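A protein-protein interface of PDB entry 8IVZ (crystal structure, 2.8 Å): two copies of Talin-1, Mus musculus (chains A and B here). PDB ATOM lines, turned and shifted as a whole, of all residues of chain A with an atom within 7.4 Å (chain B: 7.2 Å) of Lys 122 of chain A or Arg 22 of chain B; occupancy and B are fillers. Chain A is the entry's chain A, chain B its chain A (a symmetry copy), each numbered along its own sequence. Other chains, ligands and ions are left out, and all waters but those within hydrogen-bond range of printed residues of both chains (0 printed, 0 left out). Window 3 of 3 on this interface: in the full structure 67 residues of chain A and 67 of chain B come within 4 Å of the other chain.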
ATOM      1  N   GLU A 115      -2.370 -10.706 -12.295  1.00  0.00           N
ATOM      2  CA  GLU A 115      -1.812  -9.475 -12.844  1.00  0.00           C
ATOM      3  C   GLU A 115      -1.832  -9.433 -14.368  1.00  0.00           C
ATOM      4  O   GLU A 115      -2.149  -8.370 -14.926  1.00  0.00           O
ATOM      5  CB  GLU A 115      -0.390  -9.268 -12.307  1.00  0.00           C
ATOM      6  CG  GLU A 115       0.273  -7.981 -12.764  1.00  0.00           C
ATOM      7  CD  GLU A 115       1.721  -7.891 -12.326  1.00  0.00           C
ATOM      8  OE1 GLU A 115       2.222  -8.868 -11.733  1.00  0.00           O
ATOM      9  OE2 GLU A 115       2.356  -6.845 -12.575  1.00  0.00           O
ATOM     10  N   ILE A 117      -4.056 -10.473 -16.238  1.00  0.00           N
ATOM     11  CA  ILE A 117      -5.431 -10.142 -16.594  1.00  0.00           C
ATOM     12  C   ILE A 117      -5.728  -8.680 -16.290  1.00  0.00           C
ATOM     13  O   ILE A 117      -6.406  -7.996 -17.066  1.00  0.00           O
ATOM     14  CB  ILE A 117      -6.397 -11.091 -15.861  1.00  0.00           C
ATOM     15  CG1 ILE A 117      -6.280 -12.507 -16.432  1.00  0.00           C
ATOM     16  CG2 ILE A 117      -7.832 -10.584 -15.934  1.00  0.00           C
ATOM     17  CD1 ILE A 117      -7.144 -13.525 -15.726  1.00  0.00           C
ATOM     18  N   VAL A 118      -5.211  -8.171 -15.170  1.00  0.00           N
ATOM     19  CA  VAL A 118      -5.481  -6.790 -14.786  1.00  0.00           C
ATOM     20  C   VAL A 118      -4.780  -5.822 -15.733  1.00  0.00           C
ATOM     21  O   VAL A 118      -5.370  -4.827 -16.170  1.00  0.00           O
ATOM     22  CB  VAL A 118      -5.070  -6.556 -13.321  1.00  0.00           C
ATOM     23  CG1 VAL A 118      -5.307  -5.109 -12.923  1.00  0.00           C
ATOM     24  CG2 VAL A 118      -5.837  -7.492 -12.402  1.00  0.00           C
ATOM     25  N   ILE A 119      -3.518  -6.099 -16.074  1.00  0.00           N
ATOM     26  CA  ILE A 119      -2.768  -5.201 -16.949  1.00  0.00           C
ATOM     27  C   ILE A 119      -3.410  -5.132 -18.328  1.00  0.00           C
ATOM     28  O   ILE A 119      -3.553  -4.049 -18.908  1.00  0.00           O
ATOM     29  CB  ILE A 119      -1.294  -5.640 -17.032  1.00  0.00           C
ATOM     30  CG1 ILE A 119      -0.634  -5.563 -15.655  1.00  0.00           C
ATOM     31  CG2 ILE A 119      -0.535  -4.780 -18.035  1.00  0.00           C
ATOM     32  CD1 ILE A 119       0.838  -5.915 -15.664  1.00  0.00           C
ATOM     33  N   SER A 120      -3.811  -6.283 -18.874  1.00  0.00           N
ATOM     34  CA  SER A 120      -4.409  -6.297 -20.205  1.00  0.00           C
ATOM     35  C   SER A 120      -5.731  -5.541 -20.234  1.00  0.00           C
ATOM     36  O   SER A 120      -6.057  -4.903 -21.241  1.00  0.00           O
ATOM     37  CB  SER A 120      -4.608  -7.737 -20.677  1.00  0.00           C
ATOM     38  OG  SER A 120      -3.379  -8.440 -20.704  1.00  0.00           O
ATOM     39  N   ALA A 121      -6.499  -5.592 -19.145  1.00  0.00           N
ATOM     40  CA  ALA A 121      -7.771  -4.882 -19.104  1.00  0.00           C
ATOM     41  C   ALA A 121      -7.573  -3.382 -18.925  1.00  0.00           C
ATOM     42  O   ALA A 121      -8.250  -2.583 -19.580  1.00  0.00           O
ATOM     43  CB  ALA A 121      -8.653  -5.442 -17.988  1.00  0.00           C
ATOM     44  N   LYS A 122      -6.655  -2.979 -18.042  1.00  0.00           N
ATOM     45  CA  LYS A 122      -6.402  -1.554 -17.850  1.00  0.00           C
ATOM     46  C   LYS A 122      -5.768  -0.928 -19.085  1.00  0.00           C
ATOM     47  O   LYS A 122      -5.979   0.261 -19.354  1.00  0.00           O
ATOM     48  CB  LYS A 122      -5.522  -1.331 -16.618  1.00  0.00           C
ATOM     49  CG  LYS A 122      -6.169  -1.797 -15.322  1.00  0.00           C
ATOM     50  CD  LYS A 122      -5.574  -1.119 -14.095  1.00  0.00           C
ATOM     51  CE  LYS A 122      -4.226  -1.705 -13.712  1.00  0.00           C
ATOM     52  NZ  LYS A 122      -3.783  -1.207 -12.380  1.00  0.00           N
ATOM     53  N   THR A 123      -4.998  -1.707 -19.847  1.00  0.00           N
ATOM     54  CA  THR A 123      -4.468  -1.207 -21.111  1.00  0.00           C
ATOM     55  C   THR A 123      -5.582  -1.017 -22.134  1.00  0.00           C
ATOM     56  O   THR A 123      -5.554  -0.062 -22.919  1.00  0.00           O
ATOM     57  CB  THR A 123      -3.397  -2.161 -21.645  1.00  0.00           C
ATOM     58  OG1 THR A 123      -2.333  -2.269 -20.691  1.00  0.00           O
ATOM     59  CG2 THR A 123      -2.832  -1.656 -22.965  1.00  0.00           C
ATOM     60  N   MET A 124      -6.580  -1.904 -22.128  1.00  0.00           N
ATOM     61  CA  MET A 124      -7.675  -1.796 -23.087  1.00  0.00           C
ATOM     62  C   MET A 124      -8.500  -0.539 -22.849  1.00  0.00           C
ATOM     63  O   MET A 124      -8.849   0.168 -23.802  1.00  0.00           O
ATOM     64  CB  MET A 124      -8.561  -3.038 -23.015  1.00  0.00           C
ATOM     65  CG  MET A 124      -9.701  -3.040 -24.021  1.00  0.00           C
ATOM     66  SD  MET A 124     -10.996  -4.215 -23.587  1.00  0.00           S
ATOM     67  CE  MET A 124     -11.520  -3.556 -22.007  1.00  0.00           C
ATOM     68  N   LEU A 125      -8.830  -0.246 -21.587  1.00  0.00           N
ATOM     69  CA  LEU A 125      -9.564   0.979 -21.282  1.00  0.00           C
ATOM     70  C   LEU A 125      -8.751   2.212 -21.652  1.00  0.00           C
ATOM     71  O   LEU A 125      -9.298   3.197 -22.160  1.00  0.00           O
ATOM     72  CB  LEU A 125      -9.937   1.016 -19.801  1.00  0.00           C
ATOM     73  CG  LEU A 125     -10.958  -0.012 -19.322  1.00  0.00           C
ATOM     74  CD1 LEU A 125     -11.227   0.168 -17.838  1.00  0.00           C
ATOM     75  CD2 LEU A 125     -12.244   0.109 -20.122  1.00  0.00           C
ATOM     76  N   GLU A 126      -7.443   2.174 -21.395  1.00  0.00           N
ATOM     77  CA  GLU A 126      -6.591   3.304 -21.749  1.00  0.00           C
ATOM     78  C   GLU A 126      -6.575   3.529 -23.255  1.00  0.00           C
ATOM     79  O   GLU A 126      -6.653   4.673 -23.718  1.00  0.00           O
ATOM     80  CB  GLU A 126      -5.174   3.080 -21.221  1.00  0.00           C
ATOM     81  CG  GLU A 126      -4.240   4.269 -21.411  1.00  0.00           C
ATOM     82  CD  GLU A 126      -4.570   5.431 -20.491  1.00  0.00           C
ATOM     83  OE1 GLU A 126      -5.299   5.223 -19.499  1.00  0.00           O
ATOM     84  OE2 GLU A 126      -4.096   6.556 -20.760  1.00  0.00           O
ATOM     85  N   SER A 127      -6.488   2.453 -24.037  1.00  0.00           N
ATOM     86  CA  SER A 127      -6.443   2.603 -25.486  1.00  0.00           C
ATOM     87  C   SER A 127      -7.819   2.935 -26.052  1.00  0.00           C
ATOM     88  O   SER A 127      -7.947   3.824 -26.903  1.00  0.00           O
ATOM     89  CB  SER A 127      -5.881   1.332 -26.120  1.00  0.00           C
ATOM     90  OG  SER A 127      -4.710   0.914 -25.441  1.00  0.00           O
ATOM     91  N   ALA A 128      -8.861   2.238 -25.592  1.00  0.00           N
ATOM     92  CA  ALA A 128     -10.208   2.527 -26.074  1.00  0.00           C
ATOM     93  C   ALA A 128     -10.640   3.941 -25.713  1.00  0.00           C
ATOM     94  O   ALA A 128     -11.395   4.570 -26.464  1.00  0.00           O
ATOM     95  CB  ALA A 128     -11.202   1.509 -25.516  1.00  0.00           C
ATOM     96  N   SER A 161      -4.507  -5.966 -26.619  1.00  0.00           N
ATOM     97  CA  SER A 161      -4.850  -6.118 -25.210  1.00  0.00           C
ATOM     98  C   SER A 161      -5.984  -7.114 -25.008  1.00  0.00           C
ATOM     99  O   SER A 161      -6.026  -7.805 -23.984  1.00  0.00           O
ATOM    100  CB  SER A 161      -5.221  -4.762 -24.608  1.00  0.00           C
ATOM    101  OG  SER A 161      -6.318  -4.182 -25.291  1.00  0.00           O
ATOM    102  N   LEU A 165      -5.701 -10.689 -23.171  1.00  0.00           N
ATOM    103  CA  LEU A 165      -6.579 -10.914 -22.028  1.00  0.00           C
ATOM    104  C   LEU A 165      -7.265 -12.271 -22.120  1.00  0.00           C
ATOM    105  O   LEU A 165      -7.326 -13.011 -21.132  1.00  0.00           O
ATOM    106  CB  LEU A 165      -7.619  -9.794 -21.932  1.00  0.00           C
ATOM    107  CG  LEU A 165      -8.629  -9.935 -20.791  1.00  0.00           C
ATOM    108  CD1 LEU A 165      -7.906 -10.088 -19.468  1.00  0.00           C
ATOM    109  CD2 LEU A 165      -9.568  -8.744 -20.749  1.00  0.00           C
ATOM    110  N   GLN B  17     -18.063   7.047 -18.248  1.00  0.00           N
ATOM    111  CA  GLN B  17     -18.348   5.680 -17.826  1.00  0.00           C
ATOM    112  C   GLN B  17     -17.095   4.814 -17.837  1.00  0.00           C
ATOM    113  O   GLN B  17     -16.986   3.877 -17.037  1.00  0.00           O
ATOM    114  CB  GLN B  17     -19.423   5.066 -18.722  1.00  0.00           C
ATOM    115  CG  GLN B  17     -20.748   5.811 -18.719  1.00  0.00           C
ATOM    116  CD  GLN B  17     -21.705   5.297 -19.778  1.00  0.00           C
ATOM    117  OE1 GLN B  17     -21.443   4.286 -20.430  1.00  0.00           O
ATOM    118  NE2 GLN B  17     -22.820   5.997 -19.958  1.00  0.00           N
ATOM    119  N   LEU B  18     -16.141   5.109 -18.725  1.00  0.00           N
ATOM    120  CA  LEU B  18     -14.930   4.299 -18.800  1.00  0.00           C
ATOM    121  C   LEU B  18     -14.019   4.533 -17.601  1.00  0.00           C
ATOM    122  O   LEU B  18     -13.413   3.586 -17.087  1.00  0.00           O
ATOM    123  CB  LEU B  18     -14.180   4.580 -20.101  1.00  0.00           C
ATOM    124  CG  LEU B  18     -14.754   3.923 -21.356  1.00  0.00           C
ATOM    125  CD1 LEU B  18     -13.834   4.149 -22.544  1.00  0.00           C
ATOM    126  CD2 LEU B  18     -14.985   2.438 -21.123  1.00  0.00           C
ATOM    127  N   GLU B  19     -13.900   5.781 -17.144  1.00  0.00           N
ATOM    128  CA  GLU B  19     -13.063   6.047 -15.980  1.00  0.00           C
ATOM    129  C   GLU B  19     -13.726   5.608 -14.682  1.00  0.00           C
ATOM    130  O   GLU B  19     -13.045   5.499 -13.656  1.00  0.00           O
ATOM    131  CB  GLU B  19     -12.699   7.532 -15.904  1.00  0.00           C
ATOM    132  CG  GLU B  19     -13.866   8.454 -15.609  1.00  0.00           C
ATOM    133  CD  GLU B  19     -13.424   9.884 -15.369  1.00  0.00           C
ATOM    134  OE1 GLU B  19     -12.200  10.127 -15.301  1.00  0.00           O
ATOM    135  OE2 GLU B  19     -14.300  10.764 -15.249  1.00  0.00           O
ATOM    136  N   THR B  20     -15.034   5.351 -14.702  1.00  0.00           N
ATOM    137  CA  THR B  20     -15.715   4.850 -13.514  1.00  0.00           C
ATOM    138  C   THR B  20     -15.566   3.339 -13.386  1.00  0.00           C
ATOM    139  O   THR B  20     -15.333   2.826 -12.286  1.00  0.00           O
ATOM    140  CB  THR B  20     -17.194   5.241 -13.553  1.00  0.00           C
ATOM    141  OG1 THR B  20     -17.310   6.664 -13.667  1.00  0.00           O
ATOM    142  CG2 THR B  20     -17.907   4.780 -12.291  1.00  0.00           C
ATOM    143  N   VAL B  21     -15.683   2.612 -14.502  1.00  0.00           N
ATOM    144  CA  VAL B  21     -15.586   1.158 -14.466  1.00  0.00           C
ATOM    145  C   VAL B  21     -14.153   0.685 -14.262  1.00  0.00           C
ATOM    146  O   VAL B  21     -13.934  -0.484 -13.924  1.00  0.00           O
ATOM    147  CB  VAL B  21     -16.183   0.558 -15.754  1.00  0.00           C
ATOM    148  CG1 VAL B  21     -15.172   0.621 -16.896  1.00  0.00           C
ATOM    149  CG2 VAL B  21     -16.658  -0.868 -15.515  1.00  0.00           C
ATOM    150  N   ARG B  22     -13.166   1.562 -14.455  1.00  0.00           N
ATOM    151  CA  ARG B  22     -11.781   1.182 -14.208  1.00  0.00           C
ATOM    152  C   ARG B  22     -11.484   1.032 -12.722  1.00  0.00           C
ATOM    153  O   ARG B  22     -10.510   0.362 -12.359  1.00  0.00           O
ATOM    154  CB  ARG B  22     -10.831   2.208 -14.831  1.00  0.00           C
ATOM    155  CG  ARG B  22      -9.377   1.756 -14.874  1.00  0.00           C
ATOM    156  CD  ARG B  22      -8.445   2.878 -15.290  1.00  0.00           C
ATOM    157  NE  ARG B  22      -7.045   2.489 -15.146  1.00  0.00           N
ATOM    158  CZ  ARG B  22      -6.353   2.598 -14.017  1.00  0.00           C
ATOM    159  NH1 ARG B  22      -6.929   3.088 -12.928  1.00  0.00           N
ATOM    160  NH2 ARG B  22      -5.082   2.219 -13.976  1.00  0.00           N
ATOM    161  N   GLU B  23     -12.308   1.630 -11.854  1.00  0.00           N
ATOM    162  CA  GLU B  23     -12.105   1.488 -10.416  1.00  0.00           C
ATOM    163  C   GLU B  23     -12.202   0.033  -9.976  1.00  0.00           C
ATOM    164  O   GLU B  23     -11.616  -0.348  -8.956  1.00  0.00           O
ATOM    165  CB  GLU B  23     -13.118   2.347  -9.658  1.00  0.00           C
ATOM    166  CG  GLU B  23     -13.040   3.831  -9.989  1.00  0.00           C
ATOM    167  CD  GLU B  23     -14.139   4.638  -9.325  1.00  0.00           C
ATOM    168  OE1 GLU B  23     -15.062   4.025  -8.747  1.00  0.00           O
ATOM    169  OE2 GLU B  23     -14.081   5.884  -9.379  1.00  0.00           O
ATOM    170  N   LEU B  24     -12.934  -0.793 -10.727  1.00  0.00           N
ATOM    171  CA  LEU B  24     -12.980  -2.218 -10.423  1.00  0.00           C
ATOM    172  C   LEU B  24     -11.634  -2.884 -10.675  1.00  0.00           C
ATOM    173  O   LEU B  24     -11.295  -3.870 -10.009  1.00  0.00           O
ATOM    174  CB  LEU B  24     -14.066  -2.900 -11.256  1.00  0.00           C
ATOM    175  CG  LEU B  24     -15.463  -2.275 -11.226  1.00  0.00           C
ATOM    176  CD1 LEU B  24     -16.380  -2.995 -12.201  1.00  0.00           C
ATOM    177  CD2 LEU B  24     -16.040  -2.305  -9.822  1.00  0.00           C
ATOM    178  N   LEU B  25     -10.854  -2.364 -11.624  1.00  0.00           N
ATOM    179  CA  LEU B  25      -9.587  -2.991 -11.975  1.00  0.00           C
ATOM    180  C   LEU B  25      -8.457  -2.614 -11.029  1.00  0.00           C
ATOM    181  O   LEU B  25      -7.418  -3.283 -11.032  1.00  0.00           O
ATOM    182  CB  LEU B  25      -9.196  -2.620 -13.408  1.00  0.00           C
ATOM    183  CG  LEU B  25     -10.060  -3.187 -14.535  1.00  0.00           C
ATOM    184  CD1 LEU B  25      -9.671  -2.557 -15.862  1.00  0.00           C
ATOM    185  CD2 LEU B  25      -9.931  -4.700 -14.601  1.00  0.00           C
ATOM    186  N   GLU B  26      -8.630  -1.565 -10.222  1.00  0.00           N
ATOM    187  CA  GLU B  26      -7.534  -1.088  -9.386  1.00  0.00           C
ATOM    188  C   GLU B  26      -7.132  -2.129  -8.348  1.00  0.00           C
ATOM    189  O   GLU B  26      -5.955  -2.491  -8.241  1.00  0.00           O
ATOM    190  CB  GLU B  26      -7.920   0.228  -8.712  1.00  0.00           C
ATOM    191  CG  GLU B  26      -7.784   1.450  -9.609  1.00  0.00           C
ATOM    192  CD  GLU B  26      -6.339   1.767  -9.957  1.00  0.00           C
ATOM    193  OE1 GLU B  26      -5.754   1.071 -10.815  1.00  0.00           O
ATOM    194  OE2 GLU B  26      -5.783   2.714  -9.363  1.00  0.00           O
ATOM    195  N   ASN B  27      -8.096  -2.625  -7.577  1.00  0.00           N
ATOM    196  CA  ASN B  27      -7.831  -3.605  -6.525  1.00  0.00           C
ATOM    197  C   ASN B  27      -8.985  -4.592  -6.454  1.00  0.00           C
ATOM    198  O   ASN B  27      -9.896  -4.453  -5.629  1.00  0.00           O
ATOM    199  CB  ASN B  27      -7.618  -2.917  -5.174  1.00  0.00           C
ATOM    200  CG  ASN B  27      -7.030  -3.846  -4.132  1.00  0.00           C
ATOM    201  OD1 ASN B  27      -6.276  -4.763  -4.457  1.00  0.00           O
ATOM    202  ND2 ASN B  27      -7.371  -3.613  -2.870  1.00  0.00           N
ATOM    203  N   THR B  85     -14.939  -5.177 -18.841  1.00  0.00           N
ATOM    204  CA  THR B  85     -14.089  -5.050 -17.664  1.00  0.00           C
ATOM    205  C   THR B  85     -14.734  -5.648 -16.421  1.00  0.00           C
ATOM    206  O   THR B  85     -14.020  -6.132 -15.535  1.00  0.00           O
ATOM    207  CB  THR B  85     -13.743  -3.580 -17.423  1.00  0.00           C
ATOM    208  OG1 THR B  85     -14.938  -2.792 -17.455  1.00  0.00           O
ATOM    209  CG2 THR B  85     -12.791  -3.087 -18.496  1.00  0.00           C
ATOM    210  N   ALA B  88     -13.583  -9.092 -16.716  1.00  0.00           N
ATOM    211  CA  ALA B  88     -12.155  -9.225 -16.450  1.00  0.00           C
ATOM    212  C   ALA B  88     -11.839  -8.987 -14.979  1.00  0.00           C
ATOM    213  O   ALA B  88     -10.949  -9.637 -14.418  1.00  0.00           O
ATOM    214  CB  ALA B  88     -11.363  -8.261 -17.333  1.00  0.00           C
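The side-chain amino group (NZ) of Lys 122 of chain A is in salt-bridge range of the side-chain carboxylate (OE1) of Glu 26 of chain B (3.4 Å).
The guanidinium group (NH1) of Arg 22 of chain B lies within salt-bridge range of the side-chain carboxylate (OE1) of Glu 26 of chain B.
O of Ala 88 of chain B touches CG2 of Ile 117 of chain A, 3.6 Å away.
CB of Ala 121 of chain A touches CD2 of Leu 25 of chain B, 3.7 Å away.
CB of Ala 88 of chain B touches CB of Ala 121 of chain A, 3.96 Å away.
Lys 122 of chain A touches Arg 22 of chain B.
Lys 122 of chain A touches Leu 25 of chain B (CG to CD1, 3.6 Å).
Leu 125 of chain A touches Leu 18 of chain B.
Leu 125 of chain A touches Arg 22 of chain B.
Leu 125 of chain A touches Leu 25 of chain B.
Leu 125 of chain A touches Thr 85 of chain B (CD2 to CG2, 3.6 Å).
Ala 88 of chain B touches Leu 165 of chain A.
Glu 115 of chain A touches none of the printed residues of chain B.
Of the printed residues of chain B, Val 118 of chain A touches Leu 25 (3.4 Å).
Of the printed residues of chain B, Ala 121 of chain A touches Leu 25 and Ala 88.
Lys 122 of chain A touches just these residues of chain B: Arg 22 (3.4 Å), Leu 25 (3.6 Å) and Glu 26 (3.4 Å).
Printed residues of chain B within 4 Å of Leu 165 of chain A: Ala 88 (3.9 Å).
Of the printed residues of chain A, Leu 18 of chain B touches Leu 125 (3.7 Å).
Arg 22 of chain B touches just these residues of chain A: Lys 122 and Leu 125.
Asn 27 of chain B touches none of the printed residues of chain A.
Printed residues of chain A that touch a printed residue of chain B: Ile 117, Val 118, Ala 121, Lys 122, Met 124, Leu 125 and Leu 165.
Hydrophobic or aromatic side chains of chain A that line the printed part of chain B: Ile 117, Val 118, Ala 121, Met 124, Leu 125 and Leu 165.
Printed residues of chain B that touch a printed residue of chain A: Leu 18, Arg 22, Leu 25, Glu 26, Thr 85 and Ala 88.
Hydrophobic or aromatic side chains of chain B within 4 Å of the printed part of chain A: Leu 18, Leu 25 and Ala 88.
No position is printed for both chains.
Of the 13 pairs that touch across the chains among the printed residues, none has its exchanged pair printed and touching as well.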
